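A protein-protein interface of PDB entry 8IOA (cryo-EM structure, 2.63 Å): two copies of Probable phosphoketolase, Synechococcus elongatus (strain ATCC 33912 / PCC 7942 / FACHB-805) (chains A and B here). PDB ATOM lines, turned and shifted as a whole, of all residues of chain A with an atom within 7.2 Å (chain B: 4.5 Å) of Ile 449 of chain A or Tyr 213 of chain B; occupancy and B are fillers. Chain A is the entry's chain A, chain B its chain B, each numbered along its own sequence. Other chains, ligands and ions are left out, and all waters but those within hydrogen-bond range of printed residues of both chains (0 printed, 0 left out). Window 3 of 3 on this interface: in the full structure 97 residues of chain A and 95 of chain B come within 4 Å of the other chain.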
ATOM      1  N   ASP A 426      -4.656  30.115  -0.132  1.00  0.00           N
ATOM      2  CA  ASP A 426      -3.523  29.326  -0.608  1.00  0.00           C
ATOM      3  C   ASP A 426      -2.282  30.200  -0.782  1.00  0.00           C
ATOM      4  O   ASP A 426      -1.483  30.016  -1.701  1.00  0.00           O
ATOM      5  CB  ASP A 426      -3.883  28.594  -1.904  1.00  0.00           C
ATOM      6  CG  ASP A 426      -2.760  27.728  -2.420  1.00  0.00           C
ATOM      7  OD1 ASP A 426      -2.192  26.948  -1.630  1.00  0.00           O
ATOM      8  OD2 ASP A 426      -2.443  27.836  -3.621  1.00  0.00           O
ATOM      9  N   GLY A 446      -9.570  15.805   3.648  1.00  0.00           N
ATOM     10  CA  GLY A 446      -9.559  14.979   2.465  1.00  0.00           C
ATOM     11  C   GLY A 446      -8.512  13.885   2.583  1.00  0.00           C
ATOM     12  O   GLY A 446      -7.777  13.797   3.569  1.00  0.00           O
ATOM     13  N   ASP A 447      -8.462  13.043   1.553  1.00  0.00           N
ATOM     14  CA  ASP A 447      -7.472  11.978   1.543  1.00  0.00           C
ATOM     15  C   ASP A 447      -6.070  12.571   1.477  1.00  0.00           C
ATOM     16  O   ASP A 447      -5.843  13.630   0.885  1.00  0.00           O
ATOM     17  CB  ASP A 447      -7.713  11.018   0.375  1.00  0.00           C
ATOM     18  CG  ASP A 447      -7.762  11.723  -0.961  1.00  0.00           C
ATOM     19  OD1 ASP A 447      -7.599  12.956  -0.987  1.00  0.00           O
ATOM     20  OD2 ASP A 447      -7.962  11.042  -1.990  1.00  0.00           O
ATOM     21  N   ARG A 448      -5.124  11.889   2.112  1.00  0.00           N
ATOM     22  CA  ARG A 448      -3.781  12.412   2.281  1.00  0.00           C
ATOM     23  C   ARG A 448      -2.764  11.384   1.813  1.00  0.00           C
ATOM     24  O   ARG A 448      -2.996  10.174   1.890  1.00  0.00           O
ATOM     25  CB  ARG A 448      -3.520  12.788   3.744  1.00  0.00           C
ATOM     26  CG  ARG A 448      -2.493  13.886   3.940  1.00  0.00           C
ATOM     27  CD  ARG A 448      -2.570  14.465   5.345  1.00  0.00           C
ATOM     28  NE  ARG A 448      -3.874  15.055   5.623  1.00  0.00           N
ATOM     29  CZ  ARG A 448      -4.842  14.455   6.304  1.00  0.00           C
ATOM     30  NH1 ARG A 448      -4.683  13.242   6.806  1.00  0.00           N
ATOM     31  NH2 ARG A 448      -5.997  15.089   6.485  1.00  0.00           N
ATOM     32  N   ILE A 449      -1.636  11.878   1.325  1.00  0.00           N
ATOM     33  CA  ILE A 449      -0.559  11.025   0.829  1.00  0.00           C
ATOM     34  C   ILE A 449       0.677  11.313   1.669  1.00  0.00           C
ATOM     35  O   ILE A 449       0.791  12.385   2.288  1.00  0.00           O
ATOM     36  CB  ILE A 449      -0.300  11.245  -0.679  1.00  0.00           C
ATOM     37  CG1 ILE A 449       0.220  12.656  -0.940  1.00  0.00           C
ATOM     38  CG2 ILE A 449      -1.569  10.997  -1.476  1.00  0.00           C
ATOM     39  CD1 ILE A 449       0.515  12.924  -2.394  1.00  0.00           C
ATOM     40  N   PRO A 450       1.621  10.369   1.731  1.00  0.00           N
ATOM     41  CA  PRO A 450       2.811  10.582   2.572  1.00  0.00           C
ATOM     42  C   PRO A 450       3.601  11.828   2.214  1.00  0.00           C
ATOM     43  O   PRO A 450       4.203  12.444   3.103  1.00  0.00           O
ATOM     44  CB  PRO A 450       3.634   9.309   2.336  1.00  0.00           C
ATOM     45  CG  PRO A 450       2.629   8.283   1.952  1.00  0.00           C
ATOM     46  CD  PRO A 450       1.587   9.013   1.158  1.00  0.00           C
ATOM     47  N   GLU A 451       3.621  12.221   0.938  1.00  0.00           N
ATOM     48  CA  GLU A 451       4.365  13.411   0.544  1.00  0.00           C
ATOM     49  C   GLU A 451       3.795  14.673   1.179  1.00  0.00           C
ATOM     50  O   GLU A 451       4.511  15.669   1.327  1.00  0.00           O
ATOM     51  CB  GLU A 451       4.373  13.543  -0.979  1.00  0.00           C
ATOM     52  CG  GLU A 451       5.007  12.366  -1.698  1.00  0.00           C
ATOM     53  CD  GLU A 451       4.985  12.528  -3.204  1.00  0.00           C
ATOM     54  OE1 GLU A 451       4.420  13.532  -3.686  1.00  0.00           O
ATOM     55  OE2 GLU A 451       5.532  11.652  -3.906  1.00  0.00           O
ATOM     56  N   ASP A 452       2.520  14.629   1.548  1.00  0.00           N
ATOM     57  CA  ASP A 452       1.850  15.778   2.150  1.00  0.00           C
ATOM     58  C   ASP A 452       2.424  16.177   3.507  1.00  0.00           C
ATOM     59  O   ASP A 452       2.507  17.364   3.826  1.00  0.00           O
ATOM     60  CB  ASP A 452       0.348  15.509   2.279  1.00  0.00           C
ATOM     61  CG  ASP A 452      -0.359  15.491   0.938  1.00  0.00           C
ATOM     62  OD1 ASP A 452       0.301  15.767  -0.087  1.00  0.00           O
ATOM     63  OD2 ASP A 452      -1.572  15.198   0.907  1.00  0.00           O
ATOM     64  N   GLU A 453       2.820  15.190   4.304  1.00  0.00           N
ATOM     65  CA  GLU A 453       3.367  15.463   5.631  1.00  0.00           C
ATOM     66  C   GLU A 453       4.726  16.147   5.543  1.00  0.00           C
ATOM     67  O   GLU A 453       5.002  17.092   6.291  1.00  0.00           O
ATOM     68  CB  GLU A 453       3.467  14.168   6.436  1.00  0.00           C
ATOM     69  CG  GLU A 453       2.123  13.529   6.738  1.00  0.00           C
ATOM     70  CD  GLU A 453       2.234  12.357   7.692  1.00  0.00           C
ATOM     71  OE1 GLU A 453       3.367  12.033   8.108  1.00  0.00           O
ATOM     72  OE2 GLU A 453       1.191  11.759   8.026  1.00  0.00           O
ATOM     73  N   ASP A 454       5.614  15.555   4.754  1.00  0.00           N
ATOM     74  CA  ASP A 454       6.973  16.050   4.603  1.00  0.00           C
ATOM     75  C   ASP A 454       7.003  17.485   4.147  1.00  0.00           C
ATOM     76  O   ASP A 454       7.946  18.210   4.399  1.00  0.00           O
ATOM     77  CB  ASP A 454       7.755  15.167   3.625  1.00  0.00           C
ATOM     78  CG  ASP A 454       8.085  13.785   4.193  1.00  0.00           C
ATOM     79  OD1 ASP A 454       7.970  13.597   5.420  1.00  0.00           O
ATOM     80  OD2 ASP A 454       8.445  12.878   3.412  1.00  0.00           O
ATOM     81  N   GLY A 456       3.602  19.815   3.111  1.00  0.00           N
ATOM     82  CA  GLY A 456       2.553  20.670   3.614  1.00  0.00           C
ATOM     83  C   GLY A 456       2.187  20.366   5.057  1.00  0.00           C
ATOM     84  O   GLY A 456       2.594  19.368   5.642  1.00  0.00           O
ATOM     85  N   LEU A 458      -1.027  19.684   6.865  1.00  0.00           N
ATOM     86  CA  LEU A 458      -2.429  19.323   6.711  1.00  0.00           C
ATOM     87  C   LEU A 458      -2.858  18.439   7.871  1.00  0.00           C
ATOM     88  O   LEU A 458      -2.159  17.480   8.216  1.00  0.00           O
ATOM     89  CB  LEU A 458      -2.667  18.597   5.385  1.00  0.00           C
ATOM     90  CG  LEU A 458      -2.250  19.319   4.104  1.00  0.00           C
ATOM     91  CD1 LEU A 458      -2.422  18.407   2.908  1.00  0.00           C
ATOM     92  CD2 LEU A 458      -3.050  20.596   3.920  1.00  0.00           C
ATOM     93  N   ASP B 178      -6.357  22.676 -11.983  1.00  0.00           N
ATOM     94  CA  ASP B 178      -7.260  22.275 -10.911  1.00  0.00           C
ATOM     95  C   ASP B 178      -7.353  23.346  -9.834  1.00  0.00           C
ATOM     96  O   ASP B 178      -8.412  23.528  -9.224  1.00  0.00           O
ATOM     97  CB  ASP B 178      -6.815  20.945 -10.313  1.00  0.00           C
ATOM     98  CG  ASP B 178      -5.318  20.850 -10.165  1.00  0.00           C
ATOM     99  OD1 ASP B 178      -4.615  21.764 -10.637  1.00  0.00           O
ATOM    100  OD2 ASP B 178      -4.842  19.859  -9.574  1.00  0.00           O
ATOM    101  N   ASN B 211      -2.809  18.271 -12.071  1.00  0.00           N
ATOM    102  CA  ASN B 211      -1.455  17.979 -11.608  1.00  0.00           C
ATOM    103  C   ASN B 211      -1.444  17.573 -10.141  1.00  0.00           C
ATOM    104  O   ASN B 211      -0.580  16.802  -9.709  1.00  0.00           O
ATOM    105  CB  ASN B 211      -0.542  19.179 -11.851  1.00  0.00           C
ATOM    106  CG  ASN B 211      -1.195  20.491 -11.491  1.00  0.00           C
ATOM    107  OD1 ASN B 211      -2.051  20.550 -10.612  1.00  0.00           O
ATOM    108  ND2 ASN B 211      -0.797  21.556 -12.175  1.00  0.00           N
ATOM    109  N   GLY B 212      -2.385  18.088  -9.358  1.00  0.00           N
ATOM    110  CA  GLY B 212      -2.569  17.667  -7.986  1.00  0.00           C
ATOM    111  C   GLY B 212      -2.199  18.690  -6.940  1.00  0.00           C
ATOM    112  O   GLY B 212      -2.502  18.473  -5.761  1.00  0.00           O
ATOM    113  N   TYR B 213      -1.562  19.795  -7.317  1.00  0.00           N
ATOM    114  CA  TYR B 213      -1.113  20.767  -6.332  1.00  0.00           C
ATOM    115  C   TYR B 213      -1.259  22.177  -6.881  1.00  0.00           C
ATOM    116  O   TYR B 213      -1.198  22.401  -8.093  1.00  0.00           O
ATOM    117  CB  TYR B 213       0.345  20.523  -5.925  1.00  0.00           C
ATOM    118  CG  TYR B 213       0.562  19.307  -5.055  1.00  0.00           C
ATOM    119  CD1 TYR B 213       0.508  19.403  -3.674  1.00  0.00           C
ATOM    120  CD2 TYR B 213       0.835  18.068  -5.613  1.00  0.00           C
ATOM    121  CE1 TYR B 213       0.711  18.300  -2.873  1.00  0.00           C
ATOM    122  CE2 TYR B 213       1.038  16.958  -4.820  1.00  0.00           C
ATOM    123  CZ  TYR B 213       0.975  17.080  -3.451  1.00  0.00           C
ATOM    124  OH  TYR B 213       1.178  15.980  -2.652  1.00  0.00           O
ATOM    125  N   LYS B 214      -1.465  23.120  -5.970  1.00  0.00           N
ATOM    126  CA  LYS B 214      -1.327  24.543  -6.242  1.00  0.00           C
ATOM    127  C   LYS B 214       0.102  24.961  -5.898  1.00  0.00           C
ATOM    128  O   LYS B 214       1.002  24.122  -5.814  1.00  0.00           O
ATOM    129  CB  LYS B 214      -2.354  25.351  -5.447  1.00  0.00           C
ATOM    130  CG  LYS B 214      -3.673  24.674  -5.220  1.00  0.00           C
ATOM    131  CD  LYS B 214      -4.532  25.514  -4.298  1.00  0.00           C
ATOM    132  CE  LYS B 214      -5.775  24.769  -3.908  1.00  0.00           C
ATOM    133  NZ  LYS B 214      -6.345  24.122  -5.114  1.00  0.00           N
ATOM    134  N   ASN B 217      -0.516  24.052  -1.802  1.00  0.00           N
ATOM    135  CA  ASN B 217      -1.542  23.221  -1.190  1.00  0.00           C
ATOM    136  C   ASN B 217      -2.027  22.196  -2.202  1.00  0.00           C
ATOM    137  O   ASN B 217      -2.006  22.467  -3.408  1.00  0.00           O
ATOM    138  CB  ASN B 217      -2.723  24.070  -0.697  1.00  0.00           C
ATOM    139  CG  ASN B 217      -3.352  23.525   0.567  1.00  0.00           C
ATOM    140  OD1 ASN B 217      -2.682  22.898   1.386  1.00  0.00           O
ATOM    141  ND2 ASN B 217      -4.645  23.769   0.736  1.00  0.00           N
ATOM    142  N   PRO B 218      -2.447  21.014  -1.752  1.00  0.00           N
ATOM    143  CA  PRO B 218      -3.135  20.092  -2.660  1.00  0.00           C
ATOM    144  C   PRO B 218      -4.430  20.708  -3.161  1.00  0.00           C
ATOM    145  O   PRO B 218      -5.117  21.429  -2.437  1.00  0.00           O
ATOM    146  CB  PRO B 218      -3.400  18.862  -1.786  1.00  0.00           C
ATOM    147  CG  PRO B 218      -2.416  18.955  -0.688  1.00  0.00           C
ATOM    148  CD  PRO B 218      -2.220  20.414  -0.429  1.00  0.00           C
ATOM    149  N   THR B 219      -4.761  20.418  -4.413  1.00  0.00           N
ATOM    150  CA  THR B 219      -5.974  20.966  -4.993  1.00  0.00           C
ATOM    151  C   THR B 219      -7.188  20.169  -4.542  1.00  0.00           C
ATOM    152  O   THR B 219      -7.098  18.982  -4.222  1.00  0.00           O
ATOM    153  CB  THR B 219      -5.897  20.975  -6.517  1.00  0.00           C
ATOM    154  OG1 THR B 219      -5.757  19.635  -6.997  1.00  0.00           O
ATOM    155  CG2 THR B 219      -4.710  21.794  -6.972  1.00  0.00           C
ATOM    156  N   ARG B 223      -7.978  15.697  -4.587  1.00  0.00           N
ATOM    157  CA  ARG B 223      -8.114  14.971  -3.336  1.00  0.00           C
ATOM    158  C   ARG B 223      -9.528  14.468  -3.082  1.00  0.00           C
ATOM    159  O   ARG B 223      -9.826  14.021  -1.973  1.00  0.00           O
ATOM    160  CB  ARG B 223      -7.639  15.845  -2.179  1.00  0.00           C
ATOM    161  CG  ARG B 223      -6.151  16.128  -2.239  1.00  0.00           C
ATOM    162  CD  ARG B 223      -5.365  14.835  -2.378  1.00  0.00           C
ATOM    163  NE  ARG B 223      -3.996  15.061  -2.823  1.00  0.00           N
ATOM    164  CZ  ARG B 223      -2.976  15.300  -2.012  1.00  0.00           C
ATOM    165  NH1 ARG B 223      -3.137  15.370  -0.702  1.00  0.00           N
ATOM    166  NH2 ARG B 223      -1.763  15.474  -2.529  1.00  0.00           N
ATOM    167  N   LYS B 293       3.136  17.371 -11.363  1.00  0.00           N
ATOM    168  CA  LYS B 293       3.493  18.771 -11.550  1.00  0.00           C
ATOM    169  C   LYS B 293       4.983  18.893 -11.834  1.00  0.00           C
ATOM    170  O   LYS B 293       5.811  18.430 -11.044  1.00  0.00           O
ATOM    171  CB  LYS B 293       3.120  19.582 -10.315  1.00  0.00           C
ATOM    172  CG  LYS B 293       3.369  21.061 -10.484  1.00  0.00           C
ATOM    173  CD  LYS B 293       2.928  21.848  -9.271  1.00  0.00           C
ATOM    174  CE  LYS B 293       1.970  22.949  -9.668  1.00  0.00           C
ATOM    175  NZ  LYS B 293       1.721  23.897  -8.552  1.00  0.00           N
ATOM    176  N   GLY B 308       6.188  16.586  -9.276  1.00  0.00           N
ATOM    177  CA  GLY B 308       4.867  16.181  -8.829  1.00  0.00           C
ATOM    178  C   GLY B 308       4.538  16.628  -7.422  1.00  0.00           C
ATOM    179  O   GLY B 308       3.891  15.883  -6.674  1.00  0.00           O
ATOM    180  N   SER B 309       4.962  17.829  -7.043  1.00  0.00           N
ATOM    181  CA  SER B 309       4.687  18.372  -5.722  1.00  0.00           C
ATOM    182  C   SER B 309       4.474  19.872  -5.841  1.00  0.00           C
ATOM    183  O   SER B 309       4.708  20.475  -6.891  1.00  0.00           O
ATOM    184  CB  SER B 309       5.820  18.067  -4.737  1.00  0.00           C
ATOM    185  OG  SER B 309       5.520  18.572  -3.448  1.00  0.00           O
ATOM    186  N   TRP B 310       4.025  20.479  -4.741  1.00  0.00           N
ATOM    187  CA  TRP B 310       3.761  21.913  -4.742  1.00  0.00           C
ATOM    188  C   TRP B 310       5.034  22.734  -4.885  1.00  0.00           C
ATOM    189  O   TRP B 310       4.961  23.902  -5.277  1.00  0.00           O
ATOM    190  CB  TRP B 310       3.019  22.314  -3.467  1.00  0.00           C
ATOM    191  CG  TRP B 310       3.775  22.032  -2.209  1.00  0.00           C
ATOM    192  CD1 TRP B 310       3.733  20.890  -1.469  1.00  0.00           C
ATOM    193  CD2 TRP B 310       4.684  22.912  -1.539  1.00  0.00           C
ATOM    194  NE1 TRP B 310       4.561  21.001  -0.380  1.00  0.00           N
ATOM    195  CE2 TRP B 310       5.157  22.234  -0.400  1.00  0.00           C
ATOM    196  CE3 TRP B 310       5.145  24.206  -1.792  1.00  0.00           C
ATOM    197  CZ2 TRP B 310       6.068  22.806   0.483  1.00  0.00           C
ATOM    198  CZ3 TRP B 310       6.048  24.772  -0.914  1.00  0.00           C
ATOM    199  CH2 TRP B 310       6.500  24.073   0.209  1.00  0.00           C
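The backbone NH (N) of Asn 217 of chain B sits close to the side-chain carboxylate (OD1) of Asp 426 of chain A (3.4 Å). OD1 of Asp 447 of chain A lies close to O of Arg 223 of chain B (2.7 Å). OD1 of Asp 452 of chain A lies within hydrogen-bond range of OH of Tyr 213 of chain B, 2.7 Å away. The side-chain carboxylate (OD1) of Asp 452 of chain A is in salt-bridge range of the guanidinium group (NH2) of Arg 223 of chain B (3.2 Å).
N of Ile 449 of chain A is in hydrogen-bond range of OD2 of Asp 452 of chain A. The side-chain amide oxygen (OD1) of Asn 211 of chain B lies close to the backbone carbonyl oxygen (O) of Tyr 213 of chain B, 3.2 Å away. The side-chain hydroxyl (OH) of Tyr 213 of chain B lies within hydrogen-bond range of the guanidinium group (NH2) of Arg 223 of chain B, 3.0 Å away. O of Tyr 213 of chain B is in hydrogen-bond range of NZ of Lys 293 of chain B, 3.3 Å away. The backbone carbonyl oxygen (O) of Lys 214 of chain B lies within hydrogen-bond range of the side-chain amino group (NZ) of Lys 293 of chain B (2.8 Å). The backbone NH of Gly 308 of chain B is in hydrogen-bond range of the backbone carbonyl oxygen of Lys 293 of chain B.
Among the printed residues, pairs that only touch across the chains: Asp 426 of chain A with Lys 214 of chain B, Ile 449 of chain A with Tyr 213 of chain B, Ile 449 of chain A with Arg 223 of chain B, Glu 451 of chain A with Gly 308 of chain B, Gly 456 of chain A with Trp 310 of chain B, Leu 458 of chain A with Asn 217 of chain B and Leu 458 of chain A with Pro 218 of chain B.
Ile 449 of chain A touches just these residues of chain B: Tyr 213 (3.1 Å) and Arg 223 (3.4 Å). Tyr 213 of chain B touches just these residues of chain A: Ile 449 (3.1 Å) and Asp 452 (2.7 Å). No residue of chain A comes within 4 Å of Gly 212 of chain B. Of the printed residues of chain A, Trp 310 of chain B touches Gly 456 (3.8 Å). Of the printed residues of chain A, Lys 214 of chain B touches Asp 426. The nearest printed residue of chain B that does not touch Ile 449 of chain A is Gly 308 of chain B (6.2 Å). The nearest printed residue of chain A that does not touch Arg 223 of chain B is Arg 448 of chain A (4.3 Å).
Printed residues of chain B that touch a printed residue of chain A: Tyr 213, Lys 214, Asn 217, Pro 218, Arg 223, Gly 308 and Trp 310. Of the 12 printed residues of chain A, 7 touch a printed residue of chain B. Printed residues of chain A that touch a printed residue of chain B: Asp 426, Asp 447, Ile 449, Glu 451, Asp 452, Gly 456 and Leu 458. Among the printed residues, Asp or Glu carboxylates within 4 Å of a Lys or Arg side-chain nitrogen of the other chain: Asp 452 of chain A with Arg 223 of chain B.
No position is printed for both chains. Of the 11 pairs that touch across the chains among the printed residues, none has its exchanged pair printed and touching as well.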
